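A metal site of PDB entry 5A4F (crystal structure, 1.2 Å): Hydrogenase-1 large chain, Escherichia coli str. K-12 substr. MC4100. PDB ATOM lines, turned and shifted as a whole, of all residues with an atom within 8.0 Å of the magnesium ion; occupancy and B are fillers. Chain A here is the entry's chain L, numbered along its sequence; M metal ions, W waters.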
ATOM      1  N   PHE A  53     -25.529  35.082   9.527  1.00  0.00           N
ATOM      2  CA  PHE A  53     -24.664  34.939  10.708  1.00  0.00           C
ATOM      3  C   PHE A  53     -24.367  36.318  11.260  1.00  0.00           C
ATOM      4  O   PHE A  53     -24.152  37.236  10.465  1.00  0.00           O
ATOM      5  CB  PHE A  53     -23.382  34.242  10.295  1.00  0.00           C
ATOM      6  CG  PHE A  53     -22.346  34.171  11.417  1.00  0.00           C
ATOM      7  CD1 PHE A  53     -22.466  33.242  12.442  1.00  0.00           C
ATOM      8  CD2 PHE A  53     -21.236  34.979  11.430  1.00  0.00           C
ATOM      9  CE1 PHE A  53     -21.525  33.160  13.467  1.00  0.00           C
ATOM     10  CE2 PHE A  53     -20.336  34.868  12.442  1.00  0.00           C
ATOM     11  CZ  PHE A  53     -20.423  33.943  13.427  1.00  0.00           C
ATOM     12  N   GLU A  57     -21.280  34.901  19.696  1.00  0.00           N
ATOM     13  CA  GLU A  57     -20.298  34.215  20.530  1.00  0.00           C
ATOM     14  C   GLU A  57     -18.933  34.963  20.561  1.00  0.00           C
ATOM     15  O   GLU A  57     -18.186  34.898  21.538  1.00  0.00           O
ATOM     16  CB  GLU A  57     -20.100  32.784  20.112  1.00  0.00           C
ATOM     17  CG  GLU A  57     -21.389  31.946  20.274  1.00  0.00           C
ATOM     18  CD  GLU A  57     -21.466  30.740  19.379  1.00  0.00           C
ATOM     19  OE1 GLU A  57     -20.937  30.812  18.239  1.00  0.00           O
ATOM     20  OE2 GLU A  57     -22.178  29.782  19.748  1.00  0.00           O
ATOM     21  N   ILE A  75     -30.061  37.552  20.350  1.00  0.00           N
ATOM     22  CA  ILE A  75     -30.021  36.439  19.396  1.00  0.00           C
ATOM     23  C   ILE A  75     -31.333  36.376  18.678  1.00  0.00           C
ATOM     24  O   ILE A  75     -31.360  36.084  17.479  1.00  0.00           O
ATOM     25  CB  ILE A  75     -29.639  35.106  20.090  1.00  0.00           C
ATOM     26  CG1 ILE A  75     -28.163  35.128  20.445  1.00  0.00           C
ATOM     27  CG2 ILE A  75     -29.965  33.962  19.164  1.00  0.00           C
ATOM     28  CD1 ILE A  75     -27.714  34.002  21.335  1.00  0.00           C
ATOM     29  N   GLU A 347     -20.382  19.770  18.451  1.00  0.00           N
ATOM     30  CA  GLU A 347     -20.751  20.395  17.199  1.00  0.00           C
ATOM     31  C   GLU A 347     -19.652  20.173  16.153  1.00  0.00           C
ATOM     32  O   GLU A 347     -18.446  20.370  16.434  1.00  0.00           O
ATOM     33  CB  GLU A 347     -20.958  21.879  17.398  1.00  0.00           C
ATOM     34  CG  GLU A 347     -22.164  22.238  18.217  1.00  0.00           C
ATOM     35  CD  GLU A 347     -22.390  23.742  18.323  1.00  0.00           C
ATOM     36  OE1 GLU A 347     -21.536  24.382  18.980  1.00  0.00           O
ATOM     37  OE2 GLU A 347     -23.426  24.208  17.779  1.00  0.00           O
ATOM     38  N   TYR A 354     -17.266  27.448   8.831  1.00  0.00           N
ATOM     39  CA  TYR A 354     -16.446  27.736   9.991  1.00  0.00           C
ATOM     40  C   TYR A 354     -15.133  26.950   9.889  1.00  0.00           C
ATOM     41  O   TYR A 354     -15.055  25.946   9.183  1.00  0.00           O
ATOM     42  CB  TYR A 354     -17.109  27.268  11.283  1.00  0.00           C
ATOM     43  CG  TYR A 354     -18.437  27.985  11.560  1.00  0.00           C
ATOM     44  CD1 TYR A 354     -18.449  29.265  12.108  1.00  0.00           C
ATOM     45  CD2 TYR A 354     -19.630  27.450  11.198  1.00  0.00           C
ATOM     46  CE1 TYR A 354     -19.625  29.938  12.265  1.00  0.00           C
ATOM     47  CE2 TYR A 354     -20.825  28.074  11.375  1.00  0.00           C
ATOM     48  CZ  TYR A 354     -20.805  29.365  11.899  1.00  0.00           C
ATOM     49  OH  TYR A 354     -21.985  30.050  12.102  1.00  0.00           O
ATOM     50  N   PRO A 365     -19.182  22.313  23.575  1.00  0.00           N
ATOM     51  CA  PRO A 365     -19.134  23.785  23.570  1.00  0.00           C
ATOM     52  C   PRO A 365     -18.100  24.445  24.472  1.00  0.00           C
ATOM     53  O   PRO A 365     -17.674  25.549  24.184  1.00  0.00           O
ATOM     54  CB  PRO A 365     -20.568  24.144  23.983  1.00  0.00           C
ATOM     55  CG  PRO A 365     -21.402  23.006  23.442  1.00  0.00           C
ATOM     56  CD  PRO A 365     -20.549  21.808  23.742  1.00  0.00           C
ATOM     57  N   GLY A 368     -15.563  24.962  22.232  1.00  0.00           N
ATOM     58  CA  GLY A 368     -16.071  25.449  20.965  1.00  0.00           C
ATOM     59  C   GLY A 368     -15.237  26.526  20.347  1.00  0.00           C
ATOM     60  O   GLY A 368     -14.472  27.241  20.998  1.00  0.00           O
ATOM     61  N   ILE A 369     -15.387  26.645  19.020  1.00  0.00           N
ATOM     62  CA  ILE A 369     -14.681  27.642  18.216  1.00  0.00           C
ATOM     63  C   ILE A 369     -15.655  28.216  17.232  1.00  0.00           C
ATOM     64  O   ILE A 369     -16.362  27.462  16.519  1.00  0.00           O
ATOM     65  CB  ILE A 369     -13.500  27.035  17.420  1.00  0.00           C
ATOM     66  CG1 ILE A 369     -12.494  26.342  18.342  1.00  0.00           C
ATOM     67  CG2 ILE A 369     -12.786  28.114  16.608  1.00  0.00           C
ATOM     68  CD1 ILE A 369     -11.431  25.555  17.609  1.00  0.00           C
ATOM     69  N   THR A 370     -15.694  29.545  17.149  1.00  0.00           N
ATOM     70  CA  THR A 370     -16.547  30.225  16.164  1.00  0.00           C
ATOM     71  C   THR A 370     -15.690  31.150  15.331  1.00  0.00           C
ATOM     72  O   THR A 370     -15.477  32.327  15.680  1.00  0.00           O
ATOM     73  CB  THR A 370     -17.717  30.966  16.839  1.00  0.00           C
ATOM     74  OG1 THR A 370     -18.415  29.993  17.609  1.00  0.00           O
ATOM     75  CG2 THR A 370     -18.621  31.601  15.773  1.00  0.00           C
ATOM     76  N   TRP A 397     -24.437  28.390   7.398  1.00  0.00           N
ATOM     77  CA  TRP A 397     -23.927  29.099   8.595  1.00  0.00           C
ATOM     78  C   TRP A 397     -24.327  28.419   9.902  1.00  0.00           C
ATOM     79  O   TRP A 397     -23.986  28.926  10.974  1.00  0.00           O
ATOM     80  CB  TRP A 397     -24.381  30.567   8.589  1.00  0.00           C
ATOM     81  CG  TRP A 397     -23.707  31.445   7.578  1.00  0.00           C
ATOM     82  CD1 TRP A 397     -24.272  32.030   6.461  1.00  0.00           C
ATOM     83  CD2 TRP A 397     -22.331  31.802   7.579  1.00  0.00           C
ATOM     84  NE1 TRP A 397     -23.305  32.759   5.792  1.00  0.00           N
ATOM     85  CE2 TRP A 397     -22.109  32.651   6.456  1.00  0.00           C
ATOM     86  CE3 TRP A 397     -21.273  31.561   8.462  1.00  0.00           C
ATOM     87  CZ2 TRP A 397     -20.860  33.113   6.126  1.00  0.00           C
ATOM     88  CZ3 TRP A 397     -20.012  32.088   8.124  1.00  0.00           C
ATOM     89  CH2 TRP A 397     -19.835  32.831   6.976  1.00  0.00           C
ATOM     90  N   ILE A 398     -25.043  27.283   9.825  1.00  0.00           N
ATOM     91  CA  ILE A 398     -25.458  26.594  11.056  1.00  0.00           C
ATOM     92  C   ILE A 398     -24.449  25.488  11.314  1.00  0.00           C
ATOM     93  O   ILE A 398     -24.163  24.658  10.438  1.00  0.00           O
ATOM     94  CB  ILE A 398     -26.854  25.997  10.863  1.00  0.00           C
ATOM     95  CG1 ILE A 398     -27.848  27.060  10.392  1.00  0.00           C
ATOM     96  CG2 ILE A 398     -27.343  25.321  12.153  1.00  0.00           C
ATOM     97  CD1 ILE A 398     -29.201  26.554   9.983  1.00  0.00           C
ATOM     98  N   LYS A 399     -23.936  25.422  12.543  1.00  0.00           N
ATOM     99  CA  LYS A 399     -23.084  24.278  12.977  1.00  0.00           C
ATOM    100  C   LYS A 399     -23.942  23.013  13.086  1.00  0.00           C
ATOM    101  O   LYS A 399     -25.177  23.104  13.148  1.00  0.00           O
ATOM    102  CB  LYS A 399     -22.402  24.536  14.290  1.00  0.00           C
ATOM    103  CG  LYS A 399     -21.440  25.719  14.301  1.00  0.00           C
ATOM    104  CD  LYS A 399     -20.683  25.826  15.633  1.00  0.00           C
ATOM    105  CE  LYS A 399     -19.674  26.964  15.702  1.00  0.00           C
ATOM    106  NZ  LYS A 399     -19.267  27.213  17.124  1.00  0.00           N
ATOM    107  N   PRO A 401     -24.845  20.122  15.506  1.00  0.00           N
ATOM    108  CA  PRO A 401     -24.781  19.471  16.838  1.00  0.00           C
ATOM    109  C   PRO A 401     -25.202  18.023  16.738  1.00  0.00           C
ATOM    110  O   PRO A 401     -26.096  17.666  15.961  1.00  0.00           O
ATOM    111  CB  PRO A 401     -25.790  20.268  17.689  1.00  0.00           C
ATOM    112  CG  PRO A 401     -26.220  21.415  16.808  1.00  0.00           C
ATOM    113  CD  PRO A 401     -26.060  20.931  15.396  1.00  0.00           C
ATOM    114  N   GLY A 513     -28.911  25.550  25.159  1.00  0.00           N
ATOM    115  CA  GLY A 513     -27.864  25.629  26.123  1.00  0.00           C
ATOM    116  C   GLY A 513     -26.905  26.778  25.844  1.00  0.00           C
ATOM    117  O   GLY A 513     -26.631  27.085  24.656  1.00  0.00           O
ATOM    118  N   TRP A 515     -23.035  27.864  27.221  1.00  0.00           N
ATOM    119  CA  TRP A 515     -21.837  27.454  27.965  1.00  0.00           C
ATOM    120  C   TRP A 515     -20.916  28.651  28.090  1.00  0.00           C
ATOM    121  O   TRP A 515     -20.566  29.276  27.060  1.00  0.00           O
ATOM    122  CB  TRP A 515     -21.147  26.307  27.200  1.00  0.00           C
ATOM    123  CG  TRP A 515     -21.793  25.008  27.232  1.00  0.00           C
ATOM    124  CD1 TRP A 515     -21.378  23.933  27.994  1.00  0.00           C
ATOM    125  CD2 TRP A 515     -22.911  24.524  26.464  1.00  0.00           C
ATOM    126  NE1 TRP A 515     -22.192  22.820  27.757  1.00  0.00           N
ATOM    127  CE2 TRP A 515     -23.128  23.155  26.802  1.00  0.00           C
ATOM    128  CE3 TRP A 515     -23.758  25.082  25.506  1.00  0.00           C
ATOM    129  CZ2 TRP A 515     -24.121  22.407  26.248  1.00  0.00           C
ATOM    130  CZ3 TRP A 515     -24.756  24.311  24.948  1.00  0.00           C
ATOM    131  CH2 TRP A 515     -24.922  22.967  25.318  1.00  0.00           C
ATOM    132  N   TYR A 526     -18.004  32.006  25.323  1.00  0.00           N
ATOM    133  CA  TYR A 526     -19.477  31.962  25.404  1.00  0.00           C
ATOM    134  C   TYR A 526     -19.939  31.230  24.158  1.00  0.00           C
ATOM    135  O   TYR A 526     -19.859  31.801  23.074  1.00  0.00           O
ATOM    136  CB  TYR A 526     -20.042  33.380  25.508  1.00  0.00           C
ATOM    137  CG  TYR A 526     -21.406  33.408  26.138  1.00  0.00           C
ATOM    138  CD1 TYR A 526     -22.513  32.893  25.505  1.00  0.00           C
ATOM    139  CD2 TYR A 526     -21.576  33.883  27.436  1.00  0.00           C
ATOM    140  CE1 TYR A 526     -23.759  32.899  26.133  1.00  0.00           C
ATOM    141  CE2 TYR A 526     -22.830  33.899  28.060  1.00  0.00           C
ATOM    142  CZ  TYR A 526     -23.902  33.384  27.420  1.00  0.00           C
ATOM    143  OH  TYR A 526     -25.127  33.380  28.025  1.00  0.00           O
ATOM    144  N   GLN A 527     -20.395  30.008  24.326  1.00  0.00           N
ATOM    145  CA  GLN A 527     -20.854  29.215  23.233  1.00  0.00           C
ATOM    146  C   GLN A 527     -22.308  28.826  23.421  1.00  0.00           C
ATOM    147  O   GLN A 527     -22.713  28.345  24.472  1.00  0.00           O
ATOM    148  CB  GLN A 527     -19.961  27.950  23.043  1.00  0.00           C
ATOM    149  CG  GLN A 527     -18.574  28.271  22.519  1.00  0.00           C
ATOM    150  CD  GLN A 527     -18.579  28.554  21.017  1.00  0.00           C
ATOM    151  OE1 GLN A 527     -19.278  27.912  20.267  1.00  0.00           O
ATOM    152  NE2 GLN A 527     -17.749  29.448  20.582  1.00  0.00           N
ATOM    153  N   CYS A 528     -23.091  28.982  22.355  1.00  0.00           N
ATOM    154  CA  CYS A 528     -24.494  28.715  22.370  1.00  0.00           C
ATOM    155  C   CYS A 528     -24.814  27.582  21.377  1.00  0.00           C
ATOM    156  O   CYS A 528     -24.303  27.552  20.270  1.00  0.00           O
ATOM    157  CB  CYS A 528     -25.311  29.922  21.947  1.00  0.00           C
ATOM    158  SG  CYS A 528     -25.041  31.392  22.942  1.00  0.00           S
ATOM    159  N   VAL A 529     -25.654  26.658  21.806  1.00  0.00           N
ATOM    160  CA  VAL A 529     -26.232  25.634  20.912  1.00  0.00           C
ATOM    161  C   VAL A 529     -27.734  25.762  21.089  1.00  0.00           C
ATOM    162  O   VAL A 529     -28.245  25.606  22.218  1.00  0.00           O
ATOM    163  CB  VAL A 529     -25.731  24.201  21.213  1.00  0.00           C
ATOM    164  CG1 VAL A 529     -26.242  23.249  20.159  1.00  0.00           C
ATOM    165  CG2 VAL A 529     -24.237  24.141  21.339  1.00  0.00           C
ATOM    166  N   VAL A 530     -28.447  26.117  20.018  1.00  0.00           N
ATOM    167  CA  VAL A 530     -29.814  26.591  20.117  1.00  0.00           C
ATOM    168  C   VAL A 530     -30.726  25.573  19.415  1.00  0.00           C
ATOM    169  O   VAL A 530     -30.246  24.784  18.590  1.00  0.00           O
ATOM    170  CB  VAL A 530     -29.843  27.995  19.461  1.00  0.00           C
ATOM    171  CG1 VAL A 530     -31.104  28.714  19.629  1.00  0.00           C
ATOM    172  CG2 VAL A 530     -28.773  28.872  20.111  1.00  0.00           C
ATOM    173  N   THR A 533     -30.465  25.218  15.758  1.00  0.00           N
ATOM    174  CA  THR A 533     -29.168  24.687  15.367  1.00  0.00           C
ATOM    175  C   THR A 533     -29.256  23.154  15.243  1.00  0.00           C
ATOM    176  O   THR A 533     -28.735  22.568  14.276  1.00  0.00           O
ATOM    177  CB  THR A 533     -28.064  25.032  16.363  1.00  0.00           C
ATOM    178  OG1 THR A 533     -28.143  26.406  16.816  1.00  0.00           O
ATOM    179  CG2 THR A 533     -26.689  24.767  15.780  1.00  0.00           C
ATOM    180  N   CYS A 579     -31.821  32.430  15.729  1.00  0.00           N
ATOM    181  CA  CYS A 579     -31.425  31.555  16.810  1.00  0.00           C
ATOM    182  C   CYS A 579     -30.383  30.547  16.335  1.00  0.00           C
ATOM    183  O   CYS A 579     -29.399  30.297  17.045  1.00  0.00           O
ATOM    184  CB  CYS A 579     -32.634  30.805  17.330  1.00  0.00           C
ATOM    185  SG  CYS A 579     -33.486  31.634  18.658  1.00  0.00           S
ATOM    186  N   SER A 580     -30.601  29.923  15.173  1.00  0.00           N
ATOM    187  CA  SER A 580     -29.790  28.788  14.782  1.00  0.00           C
ATOM    188  C   SER A 580     -28.337  29.171  14.578  1.00  0.00           C
ATOM    189  O   SER A 580     -27.443  28.316  14.782  1.00  0.00           O
ATOM    190  CB  SER A 580     -30.330  28.137  13.521  1.00  0.00           C
ATOM    191  OG  SER A 580     -30.064  28.887  12.335  1.00  0.00           O
ATOM    192  N   THR A 581     -28.098  30.402  14.119  1.00  0.00           N
ATOM    193  CA  THR A 581     -26.801  30.881  13.718  1.00  0.00           C
ATOM    194  C   THR A 581     -26.130  31.787  14.733  1.00  0.00           C
ATOM    195  O   THR A 581     -24.908  31.756  14.909  1.00  0.00           O
ATOM    196  CB  THR A 581     -26.909  31.613  12.364  1.00  0.00           C
ATOM    197  OG1 THR A 581     -27.886  32.636  12.433  1.00  0.00           O
ATOM    198  CG2 THR A 581     -27.310  30.565  11.261  1.00  0.00           C
ATOM    199  N   HIS A 582     -26.930  32.670  15.357  1.00  0.00           N
ATOM    200  CA  HIS A 582     -26.436  33.567  16.377  1.00  0.00           C
ATOM    201  C   HIS A 582     -25.124  34.235  15.977  1.00  0.00           C
ATOM    202  O   HIS A 582     -24.212  34.368  16.821  1.00  0.00           O
ATOM    203  CB  HIS A 582     -26.433  32.902  17.797  1.00  0.00           C
ATOM    204  CG  HIS A 582     -25.877  31.509  17.844  1.00  0.00           C
ATOM    205  ND1 HIS A 582     -26.636  30.415  17.549  1.00  0.00           N
ATOM    206  CD2 HIS A 582     -24.689  31.027  18.238  1.00  0.00           C
ATOM    207  CE1 HIS A 582     -25.912  29.318  17.711  1.00  0.00           C
ATOM    208  NE2 HIS A 582     -24.722  29.660  18.115  1.00  0.00           N
ATOM    209  OXT HIS A 582     -25.068  34.766  14.810  1.00  0.00           O
HETATM  210 MG    MG M   1     -23.116  28.221  18.618  1.00  0.00          MG
HETATM  211  O   HOH W   1     -21.991  28.840  16.920  1.00  0.00           O
HETATM  212  O   HOH W   2     -24.028  26.752  17.458  1.00  0.00           O
HETATM  213  O   HOH W   3     -21.558  26.939  19.161  1.00  0.00           O
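The side-chain carboxylate of Glu 57 sits close to the side-chain amide oxygen of Gln 527. OE1 of Glu 57 sits at hydrogen-bond distance from OG1 of Thr 370 (2.7 Å). A ring nitrogen (ND1) of His 582 sits at hydrogen-bond distance from the backbone carbonyl oxygen (O) of Cys 579, 2.8 Å away.
Three residues have an atom within 4 Å of the magnesium ion: Glu 57, Cys 528 and His 582.
Water W2 binds the magnesium ion (2.1 Å). Water W3 binds the magnesium ion (2.1 Å). The magnesium ion is bound by water W1, 2.1 Å away. The backbone carbonyl oxygen (O) of Cys 528 binds the magnesium ion (2.1 Å). OE2 of Glu 57 is bound to the magnesium ion, 2.1 Å away. NE2 of His 582 is bound to the magnesium ion (2.2 Å). The magnesium ion has six donor atoms within binding distance.
Water W1 bridges OE1 of Glu 57 (2.6 Å) and NZ of Lys 399 (3.2 Å). Water W3 lies within hydrogen-bond range of the side-chain carboxylate of Glu 347 (2.6 Å), the side-chain amide oxygen of Gln 527 (2.7 Å) and the side-chain amino group of Lys 399 (3.1 Å).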
